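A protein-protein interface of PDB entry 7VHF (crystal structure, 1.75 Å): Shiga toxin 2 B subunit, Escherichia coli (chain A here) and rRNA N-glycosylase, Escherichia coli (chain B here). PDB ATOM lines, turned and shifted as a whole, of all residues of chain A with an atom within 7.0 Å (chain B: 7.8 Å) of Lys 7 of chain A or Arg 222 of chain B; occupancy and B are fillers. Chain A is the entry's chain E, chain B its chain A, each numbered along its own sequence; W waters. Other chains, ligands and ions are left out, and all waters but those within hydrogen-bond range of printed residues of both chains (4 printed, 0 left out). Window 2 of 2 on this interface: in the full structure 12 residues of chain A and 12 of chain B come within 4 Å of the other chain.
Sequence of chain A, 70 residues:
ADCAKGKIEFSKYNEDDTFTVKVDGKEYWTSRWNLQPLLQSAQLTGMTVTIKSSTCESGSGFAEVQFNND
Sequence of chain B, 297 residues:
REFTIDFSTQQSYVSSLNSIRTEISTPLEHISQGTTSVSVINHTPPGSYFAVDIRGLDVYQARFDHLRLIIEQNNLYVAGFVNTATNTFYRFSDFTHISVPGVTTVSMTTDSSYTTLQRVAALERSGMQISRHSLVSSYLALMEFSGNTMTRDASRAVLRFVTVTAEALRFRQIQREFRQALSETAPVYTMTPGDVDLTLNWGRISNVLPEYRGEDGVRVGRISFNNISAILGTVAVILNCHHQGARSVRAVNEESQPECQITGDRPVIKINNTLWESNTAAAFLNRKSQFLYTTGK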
ATOM      1  N   LYS A   5      14.523 -23.154  33.126  1.00  0.00           N
ATOM      2  CA  LYS A   5      14.011 -21.796  33.253  1.00  0.00           C
ATOM      3  C   LYS A   5      14.155 -21.116  31.906  1.00  0.00           C
ATOM      4  O   LYS A   5      15.237 -21.134  31.309  1.00  0.00           O
ATOM      5  CB  LYS A   5      14.763 -21.010  34.336  1.00  0.00           C
ATOM      6  CG  LYS A   5      14.479 -19.532  34.324  1.00  0.00           C
ATOM      7  CD  LYS A   5      14.702 -18.925  35.709  1.00  0.00           C
ATOM      8  CE  LYS A   5      14.363 -17.448  35.705  1.00  0.00           C
ATOM      9  NZ  LYS A   5      15.371 -16.632  36.444  1.00  0.00           N
ATOM     10  N   GLY A   6      13.069 -20.546  31.414  1.00  0.00           N
ATOM     11  CA  GLY A   6      13.125 -19.873  30.131  1.00  0.00           C
ATOM     12  C   GLY A   6      11.739 -19.676  29.562  1.00  0.00           C
ATOM     13  O   GLY A   6      10.739 -19.986  30.196  1.00  0.00           O
ATOM     14  N   LYS A   7      11.704 -19.136  28.346  1.00  0.00           N
ATOM     15  CA  LYS A   7      10.421 -19.050  27.669  1.00  0.00           C
ATOM     16  C   LYS A   7      10.054 -20.419  27.107  1.00  0.00           C
ATOM     17  O   LYS A   7      10.908 -21.281  26.892  1.00  0.00           O
ATOM     18  CB  LYS A   7      10.447 -18.018  26.548  1.00  0.00           C
ATOM     19  CG  LYS A   7      10.657 -16.580  27.020  1.00  0.00           C
ATOM     20  CD  LYS A   7      10.605 -15.632  25.821  1.00  0.00           C
ATOM     21  CE  LYS A   7      10.836 -14.176  26.227  1.00  0.00           C
ATOM     22  NZ  LYS A   7      10.242 -13.268  25.189  1.00  0.00           N
ATOM     23  N   ILE A   8       8.762 -20.626  26.890  1.00  0.00           N
ATOM     24  CA  ILE A   8       8.302 -21.913  26.373  1.00  0.00           C
ATOM     25  C   ILE A   8       8.530 -21.954  24.866  1.00  0.00           C
ATOM     26  O   ILE A   8       8.014 -21.115  24.124  1.00  0.00           O
ATOM     27  CB  ILE A   8       6.828 -22.167  26.727  1.00  0.00           C
ATOM     28  CG1 ILE A   8       6.673 -22.390  28.238  1.00  0.00           C
ATOM     29  CG2 ILE A   8       6.286 -23.345  25.938  1.00  0.00           C
ATOM     30  CD1 ILE A   8       5.241 -22.286  28.732  1.00  0.00           C
ATOM     31  N   GLU A   9       9.309 -22.936  24.411  1.00  0.00           N
ATOM     32  CA  GLU A   9       9.634 -22.995  22.987  1.00  0.00           C
ATOM     33  C   GLU A   9       8.489 -23.597  22.187  1.00  0.00           C
ATOM     34  O   GLU A   9       8.136 -23.095  21.114  1.00  0.00           O
ATOM     35  CB  GLU A   9      10.908 -23.802  22.767  1.00  0.00           C
ATOM     36  CG  GLU A   9      11.274 -23.893  21.300  1.00  0.00           C
ATOM     37  CD  GLU A   9      12.468 -24.788  21.043  1.00  0.00           C
ATOM     38  OE1 GLU A   9      13.233 -25.034  21.997  1.00  0.00           O
ATOM     39  OE2 GLU A   9      12.649 -25.216  19.877  1.00  0.00           O
ATOM     40  N   PHE A  10       7.913 -24.685  22.685  1.00  0.00           N
ATOM     41  CA  PHE A  10       6.676 -25.205  22.131  1.00  0.00           C
ATOM     42  C   PHE A  10       5.941 -25.935  23.242  1.00  0.00           C
ATOM     43  O   PHE A  10       6.506 -26.248  24.301  1.00  0.00           O
ATOM     44  CB  PHE A  10       6.920 -26.107  20.890  1.00  0.00           C
ATOM     45  CG  PHE A  10       7.482 -27.475  21.207  1.00  0.00           C
ATOM     46  CD1 PHE A  10       6.670 -28.494  21.677  1.00  0.00           C
ATOM     47  CD2 PHE A  10       8.823 -27.749  20.973  1.00  0.00           C
ATOM     48  CE1 PHE A  10       7.188 -29.746  21.962  1.00  0.00           C
ATOM     49  CE2 PHE A  10       9.349 -29.002  21.239  1.00  0.00           C
ATOM     50  CZ  PHE A  10       8.530 -30.001  21.740  1.00  0.00           C
ATOM     51  N   LYS A  22       8.566 -27.501  26.115  1.00  0.00           N
ATOM     52  CA  LYS A  22      10.014 -27.447  25.965  1.00  0.00           C
ATOM     53  C   LYS A  22      10.504 -26.103  26.477  1.00  0.00           C
ATOM     54  O   LYS A  22      10.053 -25.053  26.011  1.00  0.00           O
ATOM     55  CB  LYS A  22      10.420 -27.664  24.509  1.00  0.00           C
ATOM     56  CG  LYS A  22      11.912 -27.871  24.347  1.00  0.00           C
ATOM     57  CD  LYS A  22      12.269 -28.179  22.895  1.00  0.00           C
ATOM     58  CE  LYS A  22      13.785 -28.163  22.680  1.00  0.00           C
ATOM     59  NZ  LYS A  22      14.186 -29.012  21.528  1.00  0.00           N
ATOM     60  N   VAL A  23      11.417 -26.143  27.440  1.00  0.00           N
ATOM     61  CA  VAL A  23      11.967 -24.951  28.071  1.00  0.00           C
ATOM     62  C   VAL A  23      13.474 -25.127  28.132  1.00  0.00           C
ATOM     63  O   VAL A  23      13.956 -26.146  28.634  1.00  0.00           O
ATOM     64  CB  VAL A  23      11.387 -24.745  29.482  1.00  0.00           C
ATOM     65  CG1 VAL A  23      11.961 -23.469  30.142  1.00  0.00           C
ATOM     66  CG2 VAL A  23       9.850 -24.720  29.428  1.00  0.00           C
ATOM     67  N   ASP A  24      14.213 -24.149  27.606  1.00  0.00           N
ATOM     68  CA  ASP A  24      15.678 -24.152  27.672  1.00  0.00           C
ATOM     69  C   ASP A  24      16.241 -25.471  27.148  1.00  0.00           C
ATOM     70  O   ASP A  24      17.110 -26.100  27.761  1.00  0.00           O
ATOM     71  CB  ASP A  24      16.177 -23.884  29.094  1.00  0.00           C
ATOM     72  CG  ASP A  24      17.661 -23.540  29.127  1.00  0.00           C
ATOM     73  OD1 ASP A  24      18.171 -23.065  28.094  1.00  0.00           O
ATOM     74  OD2 ASP A  24      18.313 -23.782  30.158  1.00  0.00           O
ATOM     75  N   GLY A  25      15.703 -25.914  26.018  1.00  0.00           N
ATOM     76  CA  GLY A  25      16.155 -27.120  25.356  1.00  0.00           C
ATOM     77  C   GLY A  25      15.722 -28.434  25.978  1.00  0.00           C
ATOM     78  O   GLY A  25      16.138 -29.493  25.491  1.00  0.00           O
ATOM     79  N   ALA A  42       1.437 -18.611  29.130  1.00  0.00           N
ATOM     80  CA  ALA A  42       2.835 -18.257  29.345  1.00  0.00           C
ATOM     81  C   ALA A  42       3.600 -18.333  28.035  1.00  0.00           C
ATOM     82  O   ALA A  42       4.428 -17.472  27.735  1.00  0.00           O
ATOM     83  CB  ALA A  42       3.462 -19.174  30.400  1.00  0.00           C
ATOM     84  N   GLN A  43       3.289 -19.334  27.210  1.00  0.00           N
ATOM     85  CA  GLN A  43       4.000 -19.456  25.946  1.00  0.00           C
ATOM     86  C   GLN A  43       3.672 -18.293  25.020  1.00  0.00           C
ATOM     87  O   GLN A  43       4.572 -17.726  24.388  1.00  0.00           O
ATOM     88  CB  GLN A  43       3.674 -20.803  25.287  1.00  0.00           C
ATOM     89  CG  GLN A  43       4.190 -20.917  23.856  1.00  0.00           C
ATOM     90  CD  GLN A  43       3.762 -22.224  23.209  1.00  0.00           C
ATOM     91  OE1 GLN A  43       3.016 -23.008  23.808  1.00  0.00           O
ATOM     92  NE2 GLN A  43       4.239 -22.474  21.995  1.00  0.00           N
ATOM     93  N   LEU A  44       2.397 -17.891  24.948  1.00  0.00           N
ATOM     94  CA  LEU A  44       2.058 -16.948  23.898  1.00  0.00           C
ATOM     95  C   LEU A  44       2.375 -15.522  24.302  1.00  0.00           C
ATOM     96  O   LEU A  44       2.437 -14.648  23.433  1.00  0.00           O
ATOM     97  CB  LEU A  44       0.583 -17.084  23.510  1.00  0.00           C
ATOM     98  CG  LEU A  44      -0.526 -16.750  24.499  1.00  0.00           C
ATOM     99  CD1 LEU A  44      -0.996 -15.326  24.283  1.00  0.00           C
ATOM    100  CD2 LEU A  44      -1.696 -17.709  24.283  1.00  0.00           C
ATOM    101  N   THR A  45       2.583 -15.280  25.596  1.00  0.00           N
ATOM    102  CA  THR A  45       2.933 -13.962  26.110  1.00  0.00           C
ATOM    103  C   THR A  45       4.415 -13.825  26.407  1.00  0.00           C
ATOM    104  O   THR A  45       4.858 -12.733  26.785  1.00  0.00           O
ATOM    105  CB  THR A  45       2.148 -13.666  27.387  1.00  0.00           C
ATOM    106  OG1 THR A  45       2.449 -14.673  28.364  1.00  0.00           O
ATOM    107  CG2 THR A  45       0.644 -13.645  27.107  1.00  0.00           C
ATOM    108  N   GLY A  46       5.190 -14.898  26.262  1.00  0.00           N
ATOM    109  CA  GLY A  46       6.620 -14.803  26.497  1.00  0.00           C
ATOM    110  C   GLY A  46       7.015 -14.724  27.954  1.00  0.00           C
ATOM    111  O   GLY A  46       8.076 -14.181  28.276  1.00  0.00           O
ATOM    112  N   MET A  47       6.197 -15.256  28.848  1.00  0.00           N
ATOM    113  CA  MET A  47       6.603 -15.397  30.239  1.00  0.00           C
ATOM    114  C   MET A  47       7.828 -16.287  30.371  1.00  0.00           C
ATOM    115  O   MET A  47       8.025 -17.231  29.612  1.00  0.00           O
ATOM    116  CB  MET A  47       5.442 -15.980  31.040  1.00  0.00           C
ATOM    117  CG  MET A  47       4.235 -15.062  31.125  1.00  0.00           C
ATOM    118  SD  MET A  47       3.071 -15.710  32.352  1.00  0.00           S
ATOM    119  CE  MET A  47       3.270 -14.570  33.728  1.00  0.00           C
ATOM    120  N   THR A  48       8.663 -15.970  31.355  1.00  0.00           N
ATOM    121  CA  THR A  48       9.704 -16.886  31.795  1.00  0.00           C
ATOM    122  C   THR A  48       9.087 -17.878  32.765  1.00  0.00           C
ATOM    123  O   THR A  48       8.505 -17.480  33.778  1.00  0.00           O
ATOM    124  CB  THR A  48      10.855 -16.119  32.451  1.00  0.00           C
ATOM    125  OG1 THR A  48      11.478 -15.283  31.475  1.00  0.00           O
ATOM    126  CG2 THR A  48      11.889 -17.084  33.035  1.00  0.00           C
ATOM    127  N   VAL A  49       9.169 -19.156  32.450  1.00  0.00           N
ATOM    128  CA  VAL A  49       8.657 -20.178  33.357  1.00  0.00           C
ATOM    129  C   VAL A  49       9.842 -20.907  33.963  1.00  0.00           C
ATOM    130  O   VAL A  49      10.889 -21.074  33.330  1.00  0.00           O
ATOM    131  CB  VAL A  49       7.694 -21.163  32.656  1.00  0.00           C
ATOM    132  CG1 VAL A  49       6.614 -20.405  31.875  1.00  0.00           C
ATOM    133  CG2 VAL A  49       8.444 -22.137  31.761  1.00  0.00           C
ATOM    134  N   ASN A  69       6.854 -12.482  34.468  1.00  0.00           N
ATOM    135  CA  ASN A  69       6.769 -11.673  33.260  1.00  0.00           C
ATOM    136  C   ASN A  69       8.144 -11.510  32.625  1.00  0.00           C
ATOM    137  O   ASN A  69       8.275 -11.538  31.396  1.00  0.00           O
ATOM    138  CB  ASN A  69       6.148 -10.316  33.574  1.00  0.00           C
ATOM    139  CG  ASN A  69       4.643 -10.386  33.676  1.00  0.00           C
ATOM    140  OD1 ASN A  69       4.024 -11.299  33.139  1.00  0.00           O
ATOM    141  ND2 ASN A  69       4.045  -9.424  34.363  1.00  0.00           N
ATOM    142  N   ASP A  70       9.179 -11.360  33.448  1.00  0.00           N
ATOM    143  CA  ASP A  70      10.553 -11.311  32.950  1.00  0.00           C
ATOM    144  C   ASP A  70      11.401 -12.386  33.628  1.00  0.00           C
ATOM    145  O   ASP A  70      12.141 -13.111  32.965  1.00  0.00           O
ATOM    146  CB  ASP A  70      11.175  -9.930  33.181  1.00  0.00           C
ATOM    147  CG  ASP A  70      10.238  -8.799  32.805  1.00  0.00           C
ATOM    148  OD1 ASP A  70       9.930  -8.647  31.601  1.00  0.00           O
ATOM    149  OD2 ASP A  70       9.812  -8.060  33.721  1.00  0.00           O
ATOM    150  N   PRO B 193      17.322 -16.904  20.494  1.00  0.00           N
ATOM    151  CA  PRO B 193      15.872 -17.113  20.408  1.00  0.00           C
ATOM    152  C   PRO B 193      15.111 -15.808  20.336  1.00  0.00           C
ATOM    153  O   PRO B 193      14.102 -15.727  19.631  1.00  0.00           O
ATOM    154  CB  PRO B 193      15.559 -17.894  21.693  1.00  0.00           C
ATOM    155  CG  PRO B 193      16.824 -18.622  21.986  1.00  0.00           C
ATOM    156  CD  PRO B 193      17.927 -17.681  21.596  1.00  0.00           C
ATOM    157  N   GLY B 194      15.565 -14.779  21.053  1.00  0.00           N
ATOM    158  CA  GLY B 194      14.887 -13.492  20.984  1.00  0.00           C
ATOM    159  C   GLY B 194      14.955 -12.865  19.603  1.00  0.00           C
ATOM    160  O   GLY B 194      13.964 -12.302  19.121  1.00  0.00           O
ATOM    161  N   ASP B 197      12.456 -14.780  17.481  1.00  0.00           N
ATOM    162  CA  ASP B 197      11.100 -14.357  17.821  1.00  0.00           C
ATOM    163  C   ASP B 197      10.759 -13.002  17.215  1.00  0.00           C
ATOM    164  O   ASP B 197       9.626 -12.783  16.772  1.00  0.00           O
ATOM    165  CB  ASP B 197      10.948 -14.310  19.335  1.00  0.00           C
ATOM    166  CG  ASP B 197      10.430 -15.618  19.912  1.00  0.00           C
ATOM    167  OD1 ASP B 197      10.251 -15.684  21.148  1.00  0.00           O
ATOM    168  OD2 ASP B 197      10.155 -16.559  19.133  1.00  0.00           O
ATOM    169  N   LEU B 198      11.713 -12.064  17.216  1.00  0.00           N
ATOM    170  CA  LEU B 198      11.446 -10.784  16.567  1.00  0.00           C
ATOM    171  C   LEU B 198      11.090 -10.995  15.105  1.00  0.00           C
ATOM    172  O   LEU B 198      10.074 -10.467  14.612  1.00  0.00           O
ATOM    173  CB  LEU B 198      12.650  -9.846  16.688  1.00  0.00           C
ATOM    174  CG  LEU B 198      12.864  -9.165  18.033  1.00  0.00           C
ATOM    175  CD1 LEU B 198      14.223  -8.482  18.050  1.00  0.00           C
ATOM    176  CD2 LEU B 198      11.742  -8.165  18.301  1.00  0.00           C
ATOM    177  N   LEU B 200       9.907 -13.572  13.663  1.00  0.00           N
ATOM    178  CA  LEU B 200       8.621 -14.243  13.491  1.00  0.00           C
ATOM    179  C   LEU B 200       7.440 -13.339  13.817  1.00  0.00           C
ATOM    180  O   LEU B 200       6.319 -13.615  13.369  1.00  0.00           O
ATOM    181  CB  LEU B 200       8.549 -15.486  14.369  1.00  0.00           C
ATOM    182  CG  LEU B 200       9.630 -16.516  14.058  1.00  0.00           C
ATOM    183  CD1 LEU B 200       9.653 -17.543  15.180  1.00  0.00           C
ATOM    184  CD2 LEU B 200       9.415 -17.149  12.683  1.00  0.00           C
ATOM    185  N   ASN B 201       7.649 -12.304  14.618  1.00  0.00           N
ATOM    186  CA  ASN B 201       6.568 -11.420  15.023  1.00  0.00           C
ATOM    187  C   ASN B 201       6.559 -10.110  14.263  1.00  0.00           C
ATOM    188  O   ASN B 201       5.885  -9.172  14.691  1.00  0.00           O
ATOM    189  CB  ASN B 201       6.660 -11.141  16.517  1.00  0.00           C
ATOM    190  CG  ASN B 201       6.196 -12.308  17.338  1.00  0.00           C
ATOM    191  OD1 ASN B 201       5.012 -12.432  17.618  1.00  0.00           O
ATOM    192  ND2 ASN B 201       7.123 -13.173  17.725  1.00  0.00           N
ATOM    193  N   ARG B 204       3.060  -8.871  13.195  1.00  0.00           N
ATOM    194  CA  ARG B 204       2.254  -8.469  14.350  1.00  0.00           C
ATOM    195  C   ARG B 204       2.745  -7.148  14.939  1.00  0.00           C
ATOM    196  O   ARG B 204       1.947  -6.249  15.268  1.00  0.00           O
ATOM    197  CB  ARG B 204       2.290  -9.580  15.392  1.00  0.00           C
ATOM    198  CG  ARG B 204       1.656 -10.873  14.874  1.00  0.00           C
ATOM    199  CD  ARG B 204       1.965 -12.036  15.786  1.00  0.00           C
ATOM    200  NE  ARG B 204       1.221 -11.969  17.040  1.00  0.00           N
ATOM    201  CZ  ARG B 204       1.340 -12.862  18.013  1.00  0.00           C
ATOM    202  NH1 ARG B 204       2.178 -13.881  17.912  1.00  0.00           N
ATOM    203  NH2 ARG B 204       0.610 -12.726  19.115  1.00  0.00           N
ATOM    204  N   VAL B 218       4.632  -1.827  25.392  1.00  0.00           N
ATOM    205  CA  VAL B 218       4.041  -2.438  24.208  1.00  0.00           C
ATOM    206  C   VAL B 218       4.205  -3.938  24.362  1.00  0.00           C
ATOM    207  O   VAL B 218       5.301  -4.415  24.668  1.00  0.00           O
ATOM    208  CB  VAL B 218       4.703  -1.959  22.901  1.00  0.00           C
ATOM    209  CG1 VAL B 218       4.080  -2.670  21.716  1.00  0.00           C
ATOM    210  CG2 VAL B 218       4.556  -0.461  22.752  1.00  0.00           C
ATOM    211  N   ARG B 219       3.121  -4.684  24.161  1.00  0.00           N
ATOM    212  CA  ARG B 219       3.152  -6.135  24.294  1.00  0.00           C
ATOM    213  C   ARG B 219       2.536  -6.723  23.044  1.00  0.00           C
ATOM    214  O   ARG B 219       1.385  -6.421  22.724  1.00  0.00           O
ATOM    215  CB  ARG B 219       2.399  -6.597  25.549  1.00  0.00           C
ATOM    216  CG  ARG B 219       3.029  -6.097  26.843  1.00  0.00           C
ATOM    217  CD  ARG B 219       4.283  -6.893  27.196  1.00  0.00           C
ATOM    218  NE  ARG B 219       3.938  -8.211  27.726  1.00  0.00           N
ATOM    219  CZ  ARG B 219       4.034  -9.358  27.063  1.00  0.00           C
ATOM    220  NH1 ARG B 219       4.551  -9.419  25.838  1.00  0.00           N
ATOM    221  NH2 ARG B 219       3.602 -10.477  27.643  1.00  0.00           N
ATOM    222  N   VAL B 220       3.305  -7.529  22.324  1.00  0.00           N
ATOM    223  CA  VAL B 220       2.849  -8.165  21.100  1.00  0.00           C
ATOM    224  C   VAL B 220       3.265  -9.620  21.221  1.00  0.00           C
ATOM    225  O   VAL B 220       4.434  -9.945  21.019  1.00  0.00           O
ATOM    226  CB  VAL B 220       3.457  -7.523  19.846  1.00  0.00           C
ATOM    227  CG1 VAL B 220       2.994  -8.279  18.610  1.00  0.00           C
ATOM    228  CG2 VAL B 220       3.069  -6.047  19.754  1.00  0.00           C
ATOM    229  N   GLY B 221       2.322 -10.497  21.552  1.00  0.00           N
ATOM    230  CA  GLY B 221       2.677 -11.879  21.832  1.00  0.00           C
ATOM    231  C   GLY B 221       3.811 -11.999  22.831  1.00  0.00           C
ATOM    232  O   GLY B 221       3.733 -11.460  23.942  1.00  0.00           O
ATOM    233  N   ARG B 222       4.887 -12.677  22.429  1.00  0.00           N
ATOM    234  CA  ARG B 222       6.052 -12.886  23.286  1.00  0.00           C
ATOM    235  C   ARG B 222       6.985 -11.679  23.358  1.00  0.00           C
ATOM    236  O   ARG B 222       7.968 -11.730  24.108  1.00  0.00           O
ATOM    237  CB  ARG B 222       6.834 -14.118  22.808  1.00  0.00           C
ATOM    238  CG  ARG B 222       5.998 -15.403  22.705  1.00  0.00           C
ATOM    239  CD  ARG B 222       6.610 -16.409  21.746  1.00  0.00           C
ATOM    240  NE  ARG B 222       7.957 -16.869  22.091  1.00  0.00           N
ATOM    241  CZ  ARG B 222       8.236 -17.806  22.989  1.00  0.00           C
ATOM    242  NH1 ARG B 222       7.292 -18.339  23.756  1.00  0.00           N
ATOM    243  NH2 ARG B 222       9.495 -18.226  23.121  1.00  0.00           N
ATOM    244  N   ILE B 223       6.680 -10.608  22.636  1.00  0.00           N
ATOM    245  CA  ILE B 223       7.547  -9.440  22.492  1.00  0.00           C
ATOM    246  C   ILE B 223       7.085  -8.377  23.476  1.00  0.00           C
ATOM    247  O   ILE B 223       5.887  -8.073  23.554  1.00  0.00           O
ATOM    248  CB  ILE B 223       7.504  -8.893  21.050  1.00  0.00           C
ATOM    249  CG1 ILE B 223       7.845  -9.954  19.989  1.00  0.00           C
ATOM    250  CG2 ILE B 223       8.447  -7.702  20.897  1.00  0.00           C
ATOM    251  CD1 ILE B 223       9.123 -10.727  20.262  1.00  0.00           C
ATOM    252  N   SER B 224       8.022  -7.806  24.236  1.00  0.00           N
ATOM    253  CA  SER B 224       7.687  -6.719  25.140  1.00  0.00           C
ATOM    254  C   SER B 224       8.697  -5.590  24.984  1.00  0.00           C
ATOM    255  O   SER B 224       9.901  -5.838  24.884  1.00  0.00           O
ATOM    256  CB  SER B 224       7.642  -7.207  26.593  1.00  0.00           C
ATOM    257  OG  SER B 224       8.794  -7.970  26.905  1.00  0.00           O
ATOM    258  N   PHE B 225       8.188  -4.358  24.942  1.00  0.00           N
ATOM    259  CA  PHE B 225       8.996  -3.137  24.967  1.00  0.00           C
ATOM    260  C   PHE B 225       8.528  -2.267  26.123  1.00  0.00           C
ATOM    261  O   PHE B 225       7.323  -2.048  26.278  1.00  0.00           O
ATOM    262  CB  PHE B 225       8.865  -2.336  23.668  1.00  0.00           C
ATOM    263  CG  PHE B 225       9.146  -3.123  22.426  1.00  0.00           C
ATOM    264  CD1 PHE B 225      10.374  -3.730  22.235  1.00  0.00           C
ATOM    265  CD2 PHE B 225       8.195  -3.229  21.430  1.00  0.00           C
ATOM    266  CE1 PHE B 225      10.631  -4.452  21.081  1.00  0.00           C
ATOM    267  CE2 PHE B 225       8.462  -3.945  20.271  1.00  0.00           C
ATOM    268  CZ  PHE B 225       9.681  -4.549  20.104  1.00  0.00           C
ATOM    269  N   TRP B 276      -1.387  -3.330  24.138  1.00  0.00           N
ATOM    270  CA  TRP B 276      -1.394  -4.755  23.848  1.00  0.00           C
ATOM    271  C   TRP B 276      -1.875  -4.995  22.433  1.00  0.00           C
ATOM    272  O   TRP B 276      -2.840  -4.373  21.984  1.00  0.00           O
ATOM    273  CB  TRP B 276      -2.338  -5.506  24.794  1.00  0.00           C
ATOM    274  CG  TRP B 276      -1.777  -5.690  26.153  1.00  0.00           C
ATOM    275  CD1 TRP B 276      -1.780  -4.782  27.174  1.00  0.00           C
ATOM    276  CD2 TRP B 276      -1.126  -6.859  26.650  1.00  0.00           C
ATOM    277  NE1 TRP B 276      -1.164  -5.316  28.273  1.00  0.00           N
ATOM    278  CE2 TRP B 276      -0.756  -6.593  27.980  1.00  0.00           C
ATOM    279  CE3 TRP B 276      -0.822  -8.109  26.097  1.00  0.00           C
ATOM    280  CZ2 TRP B 276      -0.096  -7.530  28.775  1.00  0.00           C
ATOM    281  CZ3 TRP B 276      -0.164  -9.035  26.883  1.00  0.00           C
ATOM    282  CH2 TRP B 276       0.194  -8.740  28.209  1.00  0.00           C
ATOM    283  N   GLU B 277      -1.224  -5.922  21.744  1.00  0.00           N
ATOM    284  CA  GLU B 277      -1.871  -6.524  20.592  1.00  0.00           C
ATOM    285  C   GLU B 277      -3.168  -7.173  21.062  1.00  0.00           C
ATOM    286  O   GLU B 277      -3.156  -7.989  21.986  1.00  0.00           O
ATOM    287  CB  GLU B 277      -0.960  -7.562  19.958  1.00  0.00           C
ATOM    288  CG  GLU B 277      -1.616  -8.221  18.748  1.00  0.00           C
ATOM    289  CD  GLU B 277      -0.964  -9.523  18.417  1.00  0.00           C
ATOM    290  OE1 GLU B 277      -1.065 -10.442  19.245  1.00  0.00           O
ATOM    291  OE2 GLU B 277      -0.348  -9.627  17.329  1.00  0.00           O
ATOM    292  N   THR B 280      -3.372 -10.991  21.428  1.00  0.00           N
ATOM    293  CA  THR B 280      -2.665 -11.605  22.554  1.00  0.00           C
ATOM    294  C   THR B 280      -3.548 -11.633  23.802  1.00  0.00           C
ATOM    295  O   THR B 280      -3.696 -12.675  24.475  1.00  0.00           O
ATOM    296  CB  THR B 280      -1.371 -10.824  22.826  1.00  0.00           C
ATOM    297  OG1 THR B 280      -0.526 -10.885  21.664  1.00  0.00           O
ATOM    298  CG2 THR B 280      -0.641 -11.370  24.025  1.00  0.00           C
HETATM  299  O   HOH W   1      11.089 -13.842  22.538  1.00  0.00           O
HETATM  300  O   HOH W   2       1.675 -14.949  20.760  1.00  0.00           O
HETATM  301  O   HOH W   3      11.510 -20.353  23.830  1.00  0.00           O
HETATM  302  O   HOH W   4       5.730 -11.575  29.478  1.00  0.00           O
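Thr 280 of chain B touches Leu 44 of chain A (O to CD1, 3.8 Å).
C of Thr 45 of chain A touches CA of Arg 222 of chain B, 3.6 Å away.
Arg 222 of chain B touches Gly 46 of chain A (CG to N, 3.7 Å).
Water W1 bridges the side-chain carboxylate of Asp 197 of chain B (2.5 Å) and the side-chain amino group of Lys 7 of chain A (2.8 Å).
Water W2 lies within hydrogen-bond range of O of Leu 44 of chain A (2.8 Å) and NH2 of Arg 204 of chain B (3.0 Å).
Water W3 lies within hydrogen-bond range of NH2 of Arg 222 of chain B, O of Lys 7 of chain A and N of Glu 9 of chain A.
NH1 of Arg 222 of chain B lies within hydrogen-bond range of O of Ile 8 of chain A, 2.9 Å away.
O of Gly 221 of chain B sits close to O of Thr 45 of chain A, at 3.3 Å.
N of Arg 222 of chain B sits at hydrogen-bond distance from O of Leu 44 of chain A.
The guanidinium group (NH2) of Arg 219 of chain B sits at hydrogen-bond distance from the backbone carbonyl oxygen (O) of Thr 45 of chain A (2.7 Å).
O of Arg 222 of chain B lies within hydrogen-bond range of NZ of Lys 7 of chain A, at 3.0 Å.
The guanidinium group of Arg 222 of chain B is in hydrogen-bond range of the backbone carbonyl oxygen of Gln 43 of chain A, 2.9 Å away.
The backbone carbonyl oxygen (O) of Leu 44 of chain A sits close to the backbone carbonyl oxygen (O) of Gly 221 of chain B.
Printed residues of chain A that touch a printed residue of chain B: Lys 7, Ile 8, Gln 43, Leu 44, Thr 45 and Gly 46.
Hydrophobic or aromatic side chains of chain A that line the printed part of chain B: Leu 44.
Among the printed residues, 10 pairs touch across the chains.
Among the printed residues, no Asp or Glu carboxylate lies within 4 Å of a Lys or Arg side-chain nitrogen of the other chain.
OD1 of Asp 197 of chain B is in salt-bridge range of NE of Arg 222 of chain B, at 2.7 Å.
The guanidinium group of Arg 219 of chain B sits at hydrogen-bond distance from the backbone carbonyl oxygen of Ile 223 of chain B (3.0 Å).
The side-chain carboxylate (OE1) of Glu 277 of chain B sits at hydrogen-bond distance from the side-chain hydroxyl (OG1) of Thr 280 of chain B.
No residue of chain B comes within 4 Å of Gly 6 of chain A.
Of the printed residues of chain B, Leu 44 of chain A touches Gly 221, Arg 222 and Thr 280.
Printed residues of chain B within 4 Å of Gly 46 of chain A: Arg 222.
Leu 198 of chain B touches none of the printed residues of chain A.
Val 218 of chain B touches none of the printed residues of chain A.
Arg 222 of chain B touches just these residues of chain A: Lys 7 (3.0 Å), Ile 8 (2.9 Å), Gln 43 (2.9 Å), Leu 44 (3.3 Å), Thr 45 (3.6 Å) and Gly 46 (3.7 Å).
Printed residues of chain A within 4 Å of Thr 280 of chain B: Leu 44.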
